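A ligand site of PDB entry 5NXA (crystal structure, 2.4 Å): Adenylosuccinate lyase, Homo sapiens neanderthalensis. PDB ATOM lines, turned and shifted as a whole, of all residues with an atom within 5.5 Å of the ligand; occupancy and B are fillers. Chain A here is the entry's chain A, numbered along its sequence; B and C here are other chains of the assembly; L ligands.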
ATOM      1  N   GLU A  84      36.401 -10.006 -29.036  1.00  0.00           N
ATOM      2  CA  GLU A  84      35.820 -10.920 -28.049  1.00  0.00           C
ATOM      3  C   GLU A  84      36.206 -10.529 -26.625  1.00  0.00           C
ATOM      4  O   GLU A  84      35.381 -10.622 -25.719  1.00  0.00           O
ATOM      5  CB  GLU A  84      36.196 -12.387 -28.346  1.00  0.00           C
ATOM      6  CG  GLU A  84      35.360 -13.346 -27.521  1.00  0.00           C
ATOM      7  CD  GLU A  84      35.532 -14.809 -27.907  1.00  0.00           C
ATOM      8  OE1 GLU A  84      36.219 -15.124 -28.904  1.00  0.00           O
ATOM      9  OE2 GLU A  84      34.959 -15.664 -27.200  1.00  0.00           O
ATOM     10  N   ARG A  88      32.814  -9.948 -25.070  1.00  0.00           N
ATOM     11  CA  ARG A  88      32.496 -11.193 -24.380  1.00  0.00           C
ATOM     12  C   ARG A  88      31.400 -11.994 -25.091  1.00  0.00           C
ATOM     13  O   ARG A  88      30.628 -12.725 -24.476  1.00  0.00           O
ATOM     14  CB  ARG A  88      32.170 -10.958 -22.885  1.00  0.00           C
ATOM     15  CG  ARG A  88      33.151 -10.065 -22.124  1.00  0.00           C
ATOM     16  CD  ARG A  88      34.559 -10.651 -22.157  1.00  0.00           C
ATOM     17  NE  ARG A  88      35.538  -9.812 -21.499  1.00  0.00           N
ATOM     18  CZ  ARG A  88      35.792  -9.767 -20.185  1.00  0.00           C
ATOM     19  NH1 ARG A  88      35.098 -10.509 -19.318  1.00  0.00           N
ATOM     20  NH2 ARG A  88      36.739  -8.972 -19.726  1.00  0.00           N
ATOM     21  N   HIS A  89      31.374 -11.834 -26.410  1.00  0.00           N
ATOM     22  CA  HIS A  89      30.417 -12.533 -27.264  1.00  0.00           C
ATOM     23  C   HIS A  89      31.153 -12.949 -28.544  1.00  0.00           C
ATOM     24  O   HIS A  89      31.463 -12.090 -29.370  1.00  0.00           O
ATOM     25  CB  HIS A  89      29.263 -11.619 -27.626  1.00  0.00           C
ATOM     26  CG  HIS A  89      28.016 -12.357 -27.954  1.00  0.00           C
ATOM     27  ND1 HIS A  89      27.023 -12.508 -27.027  1.00  0.00           N
ATOM     28  CD2 HIS A  89      27.586 -12.981 -29.078  1.00  0.00           C
ATOM     29  CE1 HIS A  89      26.003 -13.159 -27.577  1.00  0.00           C
ATOM     30  NE2 HIS A  89      26.324 -13.470 -28.813  1.00  0.00           N
ATOM     31  N   ASP A  90      31.432 -14.242 -28.696  1.00  0.00           N
ATOM     32  CA  ASP A  90      32.208 -14.710 -29.847  1.00  0.00           C
ATOM     33  C   ASP A  90      31.528 -14.459 -31.195  1.00  0.00           C
ATOM     34  O   ASP A  90      32.183 -14.024 -32.148  1.00  0.00           O
ATOM     35  CB  ASP A  90      32.668 -16.179 -29.689  1.00  0.00           C
ATOM     36  CG  ASP A  90      31.506 -17.195 -29.538  1.00  0.00           C
ATOM     37  OD1 ASP A  90      30.337 -16.793 -29.414  1.00  0.00           O
ATOM     38  OD2 ASP A  90      31.770 -18.424 -29.517  1.00  0.00           O
ATOM     39  N   VAL A  91      30.212 -14.669 -31.259  1.00  0.00           N
ATOM     40  CA  VAL A  91      29.468 -14.452 -32.512  1.00  0.00           C
ATOM     41  C   VAL A  91      29.468 -12.979 -32.915  1.00  0.00           C
ATOM     42  O   VAL A  91      29.709 -12.662 -34.077  1.00  0.00           O
ATOM     43  CB  VAL A  91      28.037 -15.010 -32.453  1.00  0.00           C
ATOM     44  CG1 VAL A  91      27.227 -14.565 -33.688  1.00  0.00           C
ATOM     45  CG2 VAL A  91      28.070 -16.528 -32.352  1.00  0.00           C
ATOM     46  N   MET A  92      29.234 -12.086 -31.952  1.00  0.00           N
ATOM     47  CA  MET A  92      29.202 -10.663 -32.251  1.00  0.00           C
ATOM     48  C   MET A  92      30.579 -10.142 -32.600  1.00  0.00           C
ATOM     49  O   MET A  92      30.721  -9.276 -33.465  1.00  0.00           O
ATOM     50  CB  MET A  92      28.595  -9.857 -31.104  1.00  0.00           C
ATOM     51  CG  MET A  92      27.059  -9.903 -31.112  1.00  0.00           C
ATOM     52  SD  MET A  92      26.285  -9.355 -32.665  1.00  0.00           S
ATOM     53  CE  MET A  92      26.882  -7.645 -32.763  1.00  0.00           C
ATOM     54  N   HIS A 110      23.981 -11.087 -40.681  1.00  0.00           N
ATOM     55  CA  HIS A 110      23.267 -11.606 -39.511  1.00  0.00           C
ATOM     56  C   HIS A 110      21.838 -11.039 -39.412  1.00  0.00           C
ATOM     57  O   HIS A 110      21.202 -11.112 -38.348  1.00  0.00           O
ATOM     58  CB  HIS A 110      24.080 -11.330 -38.211  1.00  0.00           C
ATOM     59  CG  HIS A 110      23.750 -12.219 -37.048  1.00  0.00           C
ATOM     60  ND1 HIS A 110      24.005 -13.569 -37.034  1.00  0.00           N
ATOM     61  CD2 HIS A 110      23.228 -11.931 -35.825  1.00  0.00           C
ATOM     62  CE1 HIS A 110      23.644 -14.093 -35.880  1.00  0.00           C
ATOM     63  NE2 HIS A 110      23.159 -13.114 -35.125  1.00  0.00           N
ATOM     64  N   ALA A 113      18.819 -12.693 -37.410  1.00  0.00           N
ATOM     65  CA  ALA A 113      19.274 -13.969 -36.887  1.00  0.00           C
ATOM     66  C   ALA A 113      19.694 -13.854 -35.431  1.00  0.00           C
ATOM     67  O   ALA A 113      19.852 -12.774 -34.898  1.00  0.00           O
ATOM     68  CB  ALA A 113      20.417 -14.505 -37.738  1.00  0.00           C
ATOM     69  N   THR A 114      19.857 -15.019 -34.807  1.00  0.00           N
ATOM     70  CA  THR A 114      20.454 -15.147 -33.490  1.00  0.00           C
ATOM     71  C   THR A 114      21.758 -15.931 -33.626  1.00  0.00           C
ATOM     72  O   THR A 114      22.008 -16.563 -34.662  1.00  0.00           O
ATOM     73  CB  THR A 114      19.487 -15.843 -32.514  1.00  0.00           C
ATOM     74  OG1 THR A 114      19.963 -15.710 -31.170  1.00  0.00           O
ATOM     75  CG2 THR A 114      19.289 -17.329 -32.820  1.00  0.00           C
ATOM     76  N   SER A 115      22.573 -15.914 -32.586  1.00  0.00           N
ATOM     77  CA  SER A 115      23.897 -16.501 -32.617  1.00  0.00           C
ATOM     78  C   SER A 115      23.892 -17.954 -33.083  1.00  0.00           C
ATOM     79  O   SER A 115      24.752 -18.382 -33.848  1.00  0.00           O
ATOM     80  CB  SER A 115      24.557 -16.385 -31.251  1.00  0.00           C
ATOM     81  OG  SER A 115      24.732 -15.019 -30.891  1.00  0.00           O
ATOM     82  N   CYS A 116      22.887 -18.701 -32.619  1.00  0.00           N
ATOM     83  CA  CYS A 116      22.760 -20.106 -32.984  1.00  0.00           C
ATOM     84  C   CYS A 116      22.565 -20.356 -34.489  1.00  0.00           C
ATOM     85  O   CYS A 116      22.793 -21.480 -34.928  1.00  0.00           O
ATOM     86  CB  CYS A 116      21.628 -20.747 -32.183  1.00  0.00           C
ATOM     87  SG  CYS A 116      22.111 -21.120 -30.471  1.00  0.00           S
ATOM     88  N   THR A 204      15.524 -15.895 -32.240  1.00  0.00           N
ATOM     89  CA  THR A 204      16.088 -15.902 -30.887  1.00  0.00           C
ATOM     90  C   THR A 204      15.505 -17.004 -29.981  1.00  0.00           C
ATOM     91  O   THR A 204      16.250 -17.631 -29.235  1.00  0.00           O
ATOM     92  CB  THR A 204      15.858 -14.519 -30.187  1.00  0.00           C
ATOM     93  OG1 THR A 204      16.291 -13.453 -30.996  1.00  0.00           O
ATOM     94  CG2 THR A 204      16.577 -14.458 -28.829  1.00  0.00           C
ATOM     95  N   GLN A 244      15.834 -21.733 -29.042  1.00  0.00           N
ATOM     96  CA  GLN A 244      16.963 -21.062 -29.648  1.00  0.00           C
ATOM     97  C   GLN A 244      17.880 -22.060 -30.375  1.00  0.00           C
ATOM     98  O   GLN A 244      18.465 -21.737 -31.408  1.00  0.00           O
ATOM     99  CB  GLN A 244      17.769 -20.322 -28.593  1.00  0.00           C
ATOM    100  CG  GLN A 244      18.882 -19.438 -29.169  1.00  0.00           C
ATOM    101  CD  GLN A 244      19.471 -18.501 -28.139  1.00  0.00           C
ATOM    102  OE1 GLN A 244      20.461 -18.826 -27.479  1.00  0.00           O
ATOM    103  NE2 GLN A 244      18.835 -17.350 -27.956  1.00  0.00           N
ATOM    104  N   ARG A 332      16.610 -22.375 -23.938  1.00  0.00           N
ATOM    105  CA  ARG A 332      18.067 -22.600 -23.970  1.00  0.00           C
ATOM    106  C   ARG A 332      18.765 -22.038 -22.735  1.00  0.00           C
ATOM    107  O   ARG A 332      18.417 -20.956 -22.296  1.00  0.00           O
ATOM    108  CB  ARG A 332      18.669 -21.763 -25.111  1.00  0.00           C
ATOM    109  CG  ARG A 332      19.965 -22.110 -25.543  1.00  0.00           C
ATOM    110  CD  ARG A 332      21.090 -21.320 -24.909  1.00  0.00           C
ATOM    111  NE  ARG A 332      22.266 -21.989 -25.414  1.00  0.00           N
ATOM    112  CZ  ARG A 332      22.953 -21.683 -26.532  1.00  0.00           C
ATOM    113  NH1 ARG A 332      22.615 -20.658 -27.298  1.00  0.00           N
ATOM    114  NH2 ARG A 332      23.998 -22.420 -26.846  1.00  0.00           N
ATOM    115  N   LEU A 334      23.051 -21.545 -21.564  1.00  0.00           N
ATOM    116  CA  LEU A 334      24.375 -21.544 -22.180  1.00  0.00           C
ATOM    117  C   LEU A 334      25.366 -22.489 -21.508  1.00  0.00           C
ATOM    118  O   LEU A 334      26.521 -22.575 -21.927  1.00  0.00           O
ATOM    119  CB  LEU A 334      24.932 -20.120 -22.181  1.00  0.00           C
ATOM    120  CG  LEU A 334      26.032 -19.815 -23.188  1.00  0.00           C
ATOM    121  CD1 LEU A 334      25.457 -19.576 -24.579  1.00  0.00           C
ATOM    122  CD2 LEU A 334      26.843 -18.619 -22.687  1.00  0.00           C
ATOM    123  N   SER A 337      27.448 -24.858 -23.793  1.00  0.00           N
ATOM    124  CA  SER A 337      28.377 -24.409 -24.828  1.00  0.00           C
ATOM    125  C   SER A 337      29.803 -24.914 -24.649  1.00  0.00           C
ATOM    126  O   SER A 337      30.361 -25.530 -25.554  1.00  0.00           O
ATOM    127  CB  SER A 337      28.338 -22.884 -24.927  1.00  0.00           C
ATOM    128  OG  SER A 337      29.284 -22.409 -25.853  1.00  0.00           O
ATOM    129  N   ALA A 338      30.397 -24.660 -23.484  1.00  0.00           N
ATOM    130  CA  ALA A 338      31.805 -25.050 -23.252  1.00  0.00           C
ATOM    131  C   ALA A 338      31.971 -26.573 -23.294  1.00  0.00           C
ATOM    132  O   ALA A 338      32.938 -27.078 -23.868  1.00  0.00           O
ATOM    133  CB  ALA A 338      32.291 -24.511 -21.906  1.00  0.00           C
ATOM    134  N   ARG A 341      32.062 -27.798 -26.841  1.00  0.00           N
ATOM    135  CA  ARG A 341      33.350 -27.516 -27.511  1.00  0.00           C
ATOM    136  C   ARG A 341      34.363 -28.632 -27.246  1.00  0.00           C
ATOM    137  O   ARG A 341      35.218 -28.904 -28.089  1.00  0.00           O
ATOM    138  CB  ARG A 341      33.968 -26.195 -27.029  1.00  0.00           C
ATOM    139  CG  ARG A 341      33.259 -24.916 -27.424  1.00  0.00           C
ATOM    140  CD  ARG A 341      33.982 -23.733 -26.777  1.00  0.00           C
ATOM    141  NE  ARG A 341      33.191 -22.503 -26.677  1.00  0.00           N
ATOM    142  CZ  ARG A 341      33.193 -21.486 -27.552  1.00  0.00           C
ATOM    143  NH1 ARG A 341      33.986 -21.496 -28.620  1.00  0.00           N
ATOM    144  NH2 ARG A 341      32.443 -20.409 -27.325  1.00  0.00           N
ATOM    145  N   ARG B  23      41.547 -21.328 -24.979  1.00  0.00           N
ATOM    146  CA  ARG B  23      40.402 -20.514 -24.554  1.00  0.00           C
ATOM    147  C   ARG B  23      40.259 -20.361 -23.041  1.00  0.00           C
ATOM    148  O   ARG B  23      40.001 -19.272 -22.552  1.00  0.00           O
ATOM    149  CB  ARG B  23      39.128 -21.132 -25.152  1.00  0.00           C
ATOM    150  CG  ARG B  23      37.945 -20.209 -25.156  1.00  0.00           C
ATOM    151  CD  ARG B  23      36.744 -20.851 -25.848  1.00  0.00           C
ATOM    152  NE  ARG B  23      35.523 -20.179 -25.400  1.00  0.00           N
ATOM    153  CZ  ARG B  23      35.149 -18.955 -25.767  1.00  0.00           C
ATOM    154  NH1 ARG B  23      35.865 -18.267 -26.659  1.00  0.00           N
ATOM    155  NH2 ARG B  23      34.036 -18.427 -25.275  1.00  0.00           N
ATOM    156  N   TYR B  24      40.457 -21.450 -22.297  1.00  0.00           N
ATOM    157  CA  TYR B  24      40.020 -21.520 -20.913  1.00  0.00           C
ATOM    158  C   TYR B  24      41.118 -21.456 -19.854  1.00  0.00           C
ATOM    159  O   TYR B  24      41.112 -20.563 -19.008  1.00  0.00           O
ATOM    160  CB  TYR B  24      39.176 -22.788 -20.720  1.00  0.00           C
ATOM    161  CG  TYR B  24      37.871 -22.760 -21.483  1.00  0.00           C
ATOM    162  CD1 TYR B  24      37.029 -21.653 -21.417  1.00  0.00           C
ATOM    163  CD2 TYR B  24      37.475 -23.825 -22.267  1.00  0.00           C
ATOM    164  CE1 TYR B  24      35.835 -21.618 -22.119  1.00  0.00           C
ATOM    165  CE2 TYR B  24      36.288 -23.784 -22.972  1.00  0.00           C
ATOM    166  CZ  TYR B  24      35.480 -22.677 -22.897  1.00  0.00           C
ATOM    167  OH  TYR B  24      34.305 -22.652 -23.606  1.00  0.00           O
ATOM    168  N   LYS B 298      19.450  -6.884 -21.715  1.00  0.00           N
ATOM    169  CA  LYS B 298      19.538  -8.272 -21.269  1.00  0.00           C
ATOM    170  C   LYS B 298      20.879  -8.589 -20.636  1.00  0.00           C
ATOM    171  O   LYS B 298      21.912  -8.404 -21.246  1.00  0.00           O
ATOM    172  CB  LYS B 298      19.243  -9.237 -22.418  1.00  0.00           C
ATOM    173  CG  LYS B 298      19.153 -10.698 -22.032  1.00  0.00           C
ATOM    174  CD  LYS B 298      18.482 -11.494 -23.116  1.00  0.00           C
ATOM    175  CE  LYS B 298      17.745 -12.693 -22.583  1.00  0.00           C
ATOM    176  NZ  LYS B 298      18.451 -13.941 -22.885  1.00  0.00           N
ATOM    177  N   ASN B 300      22.924 -11.643 -18.898  1.00  0.00           N
ATOM    178  CA  ASN B 300      22.967 -13.099 -18.753  1.00  0.00           C
ATOM    179  C   ASN B 300      24.101 -13.526 -17.839  1.00  0.00           C
ATOM    180  O   ASN B 300      25.165 -12.924 -17.869  1.00  0.00           O
ATOM    181  CB  ASN B 300      23.148 -13.772 -20.116  1.00  0.00           C
ATOM    182  CG  ASN B 300      22.026 -13.466 -21.078  1.00  0.00           C
ATOM    183  OD1 ASN B 300      20.865 -13.478 -20.703  1.00  0.00           O
ATOM    184  ND2 ASN B 300      22.365 -13.222 -22.318  1.00  0.00           N
ATOM    185  N   MET B 302      26.571 -15.558 -17.903  1.00  0.00           N
ATOM    186  CA  MET B 302      27.359 -16.406 -18.818  1.00  0.00           C
ATOM    187  C   MET B 302      28.612 -17.010 -18.188  1.00  0.00           C
ATOM    188  O   MET B 302      29.034 -18.107 -18.591  1.00  0.00           O
ATOM    189  CB  MET B 302      27.722 -15.664 -20.123  1.00  0.00           C
ATOM    190  CG  MET B 302      28.559 -14.406 -19.975  1.00  0.00           C
ATOM    191  SD  MET B 302      30.352 -14.649 -20.026  1.00  0.00           S
ATOM    192  CE  MET B 302      30.681 -14.481 -21.797  1.00  0.00           C
ATOM    193  N   ARG B 306      29.134 -20.986 -17.951  1.00  0.00           N
ATOM    194  CA  ARG B 306      30.367 -21.655 -18.371  1.00  0.00           C
ATOM    195  C   ARG B 306      30.945 -22.535 -17.262  1.00  0.00           C
ATOM    196  O   ARG B 306      31.467 -23.623 -17.534  1.00  0.00           O
ATOM    197  CB  ARG B 306      31.393 -20.628 -18.804  1.00  0.00           C
ATOM    198  CG  ARG B 306      32.715 -21.226 -19.290  1.00  0.00           C
ATOM    199  CD  ARG B 306      33.739 -20.164 -19.550  1.00  0.00           C
ATOM    200  NE  ARG B 306      33.250 -19.228 -20.550  1.00  0.00           N
ATOM    201  CZ  ARG B 306      33.664 -17.983 -20.704  1.00  0.00           C
ATOM    202  NH1 ARG B 306      34.636 -17.482 -19.947  1.00  0.00           N
ATOM    203  NH2 ARG B 306      33.106 -17.238 -21.668  1.00  0.00           N
ATOM    204  N   LEU B 487      37.509 -13.497 -21.880  1.00  0.00           N
ATOM    205  CA  LEU B 487      36.381 -13.846 -22.706  1.00  0.00           C
ATOM    206  C   LEU B 487      35.238 -14.228 -21.837  1.00  0.00           C
ATOM    207  O   LEU B 487      34.325 -14.842 -22.304  1.00  0.00           O
ATOM    208  CB  LEU B 487      36.721 -15.018 -23.612  1.00  0.00           C
ATOM    209  CG  LEU B 487      37.720 -16.038 -23.088  1.00  0.00           C
ATOM    210  CD1 LEU B 487      37.020 -17.125 -22.308  1.00  0.00           C
ATOM    211  CD2 LEU B 487      38.460 -16.620 -24.257  1.00  0.00           C
ATOM    212  N   THR C 161      15.823 -17.450 -22.280  1.00  0.00           N
ATOM    213  CA  THR C 161      17.149 -17.952 -22.613  1.00  0.00           C
ATOM    214  C   THR C 161      18.119 -17.504 -21.525  1.00  0.00           C
ATOM    215  O   THR C 161      18.033 -16.380 -21.057  1.00  0.00           O
ATOM    216  CB  THR C 161      17.600 -17.455 -24.009  1.00  0.00           C
ATOM    217  OG1 THR C 161      17.728 -16.039 -24.026  1.00  0.00           O
ATOM    218  CG2 THR C 161      16.582 -17.859 -25.059  1.00  0.00           C
ATOM    219  N   HIS C 162      19.024 -18.380 -21.105  1.00  0.00           N
ATOM    220  CA  HIS C 162      19.851 -18.178 -19.881  1.00  0.00           C
ATOM    221  C   HIS C 162      18.976 -17.992 -18.631  1.00  0.00           C
ATOM    222  O   HIS C 162      19.443 -17.468 -17.612  1.00  0.00           O
ATOM    223  CB  HIS C 162      20.786 -16.959 -20.010  1.00  0.00           C
ATOM    224  CG  HIS C 162      21.545 -16.878 -21.301  1.00  0.00           C
ATOM    225  ND1 HIS C 162      22.909 -17.006 -21.346  1.00  0.00           N
ATOM    226  CD2 HIS C 162      21.144 -16.586 -22.562  1.00  0.00           C
ATOM    227  CE1 HIS C 162      23.324 -16.854 -22.598  1.00  0.00           C
ATOM    228  NE2 HIS C 162      22.277 -16.615 -23.357  1.00  0.00           N
HETATM  229  P1  LIG L   1      31.503 -20.558 -23.584  1.00  0.00           P
HETATM  230  O1  LIG L   1      31.424 -21.751 -24.477  1.00  0.00           O
HETATM  231  O2  LIG L   1      32.896 -20.293 -23.122  1.00  0.00           O
HETATM  232  O3  LIG L   1      30.465 -20.400 -22.481  1.00  0.00           O
HETATM  233  O4  LIG L   1      31.270 -19.398 -24.645  1.00  0.00           O
HETATM  234  C1  LIG L   1      29.960 -18.898 -24.742  1.00  0.00           C
HETATM  235  C2  LIG L   1      29.943 -17.870 -25.838  1.00  0.00           C
HETATM  236  O5  LIG L   1      28.591 -17.847 -26.245  1.00  0.00           O
HETATM  237  C3  LIG L   1      28.183 -16.499 -26.370  1.00  0.00           C
HETATM  238  N1  LIG L   1      26.723 -16.281 -26.096  1.00  0.00           N
HETATM  239  C4  LIG L   1      25.758 -16.572 -26.951  1.00  0.00           C
HETATM  240  O6  LIG L   1      22.953 -17.334 -27.781  1.00  0.00           O
HETATM  241  N2  LIG L   1      25.921 -17.196 -28.148  1.00  0.00           N
HETATM  242  C5  LIG L   1      23.225 -16.339 -27.113  1.00  0.00           C
HETATM  243  N3  LIG L   1      22.663 -15.111 -27.131  1.00  0.00           N
HETATM  244  C6  LIG L   1      21.665 -14.602 -28.054  1.00  0.00           C
HETATM  245  C7  LIG L   1      22.268 -13.723 -29.145  1.00  0.00           C
HETATM  246  C8  LIG L   1      20.611 -13.829 -27.261  1.00  0.00           C
HETATM  247  C9  LIG L   1      20.312 -14.523 -25.944  1.00  0.00           C
HETATM  248  O7  LIG L   1      22.970 -12.708 -28.843  1.00  0.00           O
HETATM  249  O8  LIG L   1      22.051 -14.027 -30.332  1.00  0.00           O
HETATM  250  O9  LIG L   1      20.122 -13.840 -24.926  1.00  0.00           O
HETATM  251  O10 LIG L   1      20.290 -15.746 -25.912  1.00  0.00           O
HETATM  252  C10 LIG L   1      24.468 -16.244 -26.368  1.00  0.00           C
HETATM  253  N4  LIG L   1      24.723 -15.646 -25.212  1.00  0.00           N
HETATM  254  C11 LIG L   1      26.089 -15.697 -25.026  1.00  0.00           C
HETATM  255  C12 LIG L   1      29.159 -15.584 -25.608  1.00  0.00           C
HETATM  256  O11 LIG L   1      28.743 -14.974 -24.370  1.00  0.00           O
HETATM  257  C13 LIG L   1      30.367 -16.452 -25.370  1.00  0.00           C
HETATM  258  O12 LIG L   1      31.496 -15.863 -26.067  1.00  0.00           O
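Residues that only touch the ligand: Glu 84, Leu 334 and Met 302 of chain B.
20 residues have an atom within 4 Å of the ligand: Glu 84, Arg 88, His 89, Asp 90, Thr 114, Ser 115, Gln 244, Arg 332, Leu 334, Ser 337, Ala 338, Arg 341, Arg 23 of chain B, Tyr 24 of chain B, Lys 298 of chain B, Asn 300 of chain B, Met 302 of chain B, Arg 306 of chain B, Thr 161 of chain C and His 162 of chain C.
OD1 of Asn 300 of chain B is in hydrogen-bond range of NZ of Lys 298 of chain B (3.3 Å).
The backbone carbonyl oxygen of Leu 487 of chain B lies within hydrogen-bond range of the guanidinium group of Arg 306 of chain B, at 2.8 Å.
A ring nitrogen (NE2) of His 89 sits at hydrogen-bond distance from the side-chain hydroxyl of Ser 115.
The side-chain amide oxygen of Gln 244 lies within hydrogen-bond range of the guanidinium group of Arg 332 (2.8 Å).
The side-chain carboxylate of Asp 90 lies within salt-bridge range of the guanidinium group of Arg 341 (3.0 Å).
OE2 of Glu 84 lies within salt-bridge range of NH1 of Arg 23 of chain B (2.8 Å).
N of His 162 of chain C lies within hydrogen-bond range of O of Arg 332, at 2.9 Å.
The guanidinium group (NH1) of Arg 332 sits at hydrogen-bond distance from the side-chain sulfur (SG) of Cys 116.
OG of Ser 337 is in hydrogen-bond range of O1 of the ligand, 2.6 Å away.
An oxygen (O9) of the ligand is in salt-bridge range of the side-chain amino group of Lys 298 of chain B (2.6 Å).
The side-chain hydroxyl (OH) of Tyr 24 of chain B is in hydrogen-bond range of an oxygen (O2) of the ligand (2.8 Å).
O2 of the ligand is in salt-bridge range of NE of Arg 306 of chain B (2.8 Å).
The side-chain hydroxyl (OG1) of Thr 114 is in hydrogen-bond range of an oxygen (O8) of the ligand.
The backbone NH (N) of Ser 115 is in hydrogen-bond range of an oxygen (O8) of the ligand, at 3.0 Å.
OG of Ser 115 is in hydrogen-bond range of O8 of the ligand (2.9 Å).
OE1 of Gln 244 sits close to O6 of the ligand (2.9 Å).
The guanidinium group (NE) of Arg 341 lies within salt-bridge range of an oxygen (O1) of the ligand, at 2.9 Å.
The backbone carbonyl oxygen (O) of Arg 88 sits at hydrogen-bond distance from an oxygen (O11) of the ligand (2.9 Å).
The guanidinium group (NH2) of Arg 23 of chain B is in salt-bridge range of an oxygen (O2) of the ligand, 3.1 Å away.
The backbone NH (N) of Asp 90 lies within hydrogen-bond range of an oxygen (O12) of the ligand.
OG1 of Thr 161 of chain C lies within hydrogen-bond range of O10 of the ligand.
NE2 of His 162 of chain C sits close to N4 of the ligand (3.2 Å).
An oxygen (O1) of the ligand sits at hydrogen-bond distance from the backbone NH (N) of Ala 338 (3.2 Å).
A ring nitrogen (NE2) of His 89 sits close to an oxygen (O7) of the ligand (3.4 Å).
The guanidinium group (NH1) of Arg 332 is in hydrogen-bond range of an oxygen (O6) of the ligand (3.4 Å).
An oxygen (O9) of the ligand sits at hydrogen-bond distance from the side-chain amide nitrogen of Asn 300 of chain B, at 3.5 Å.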
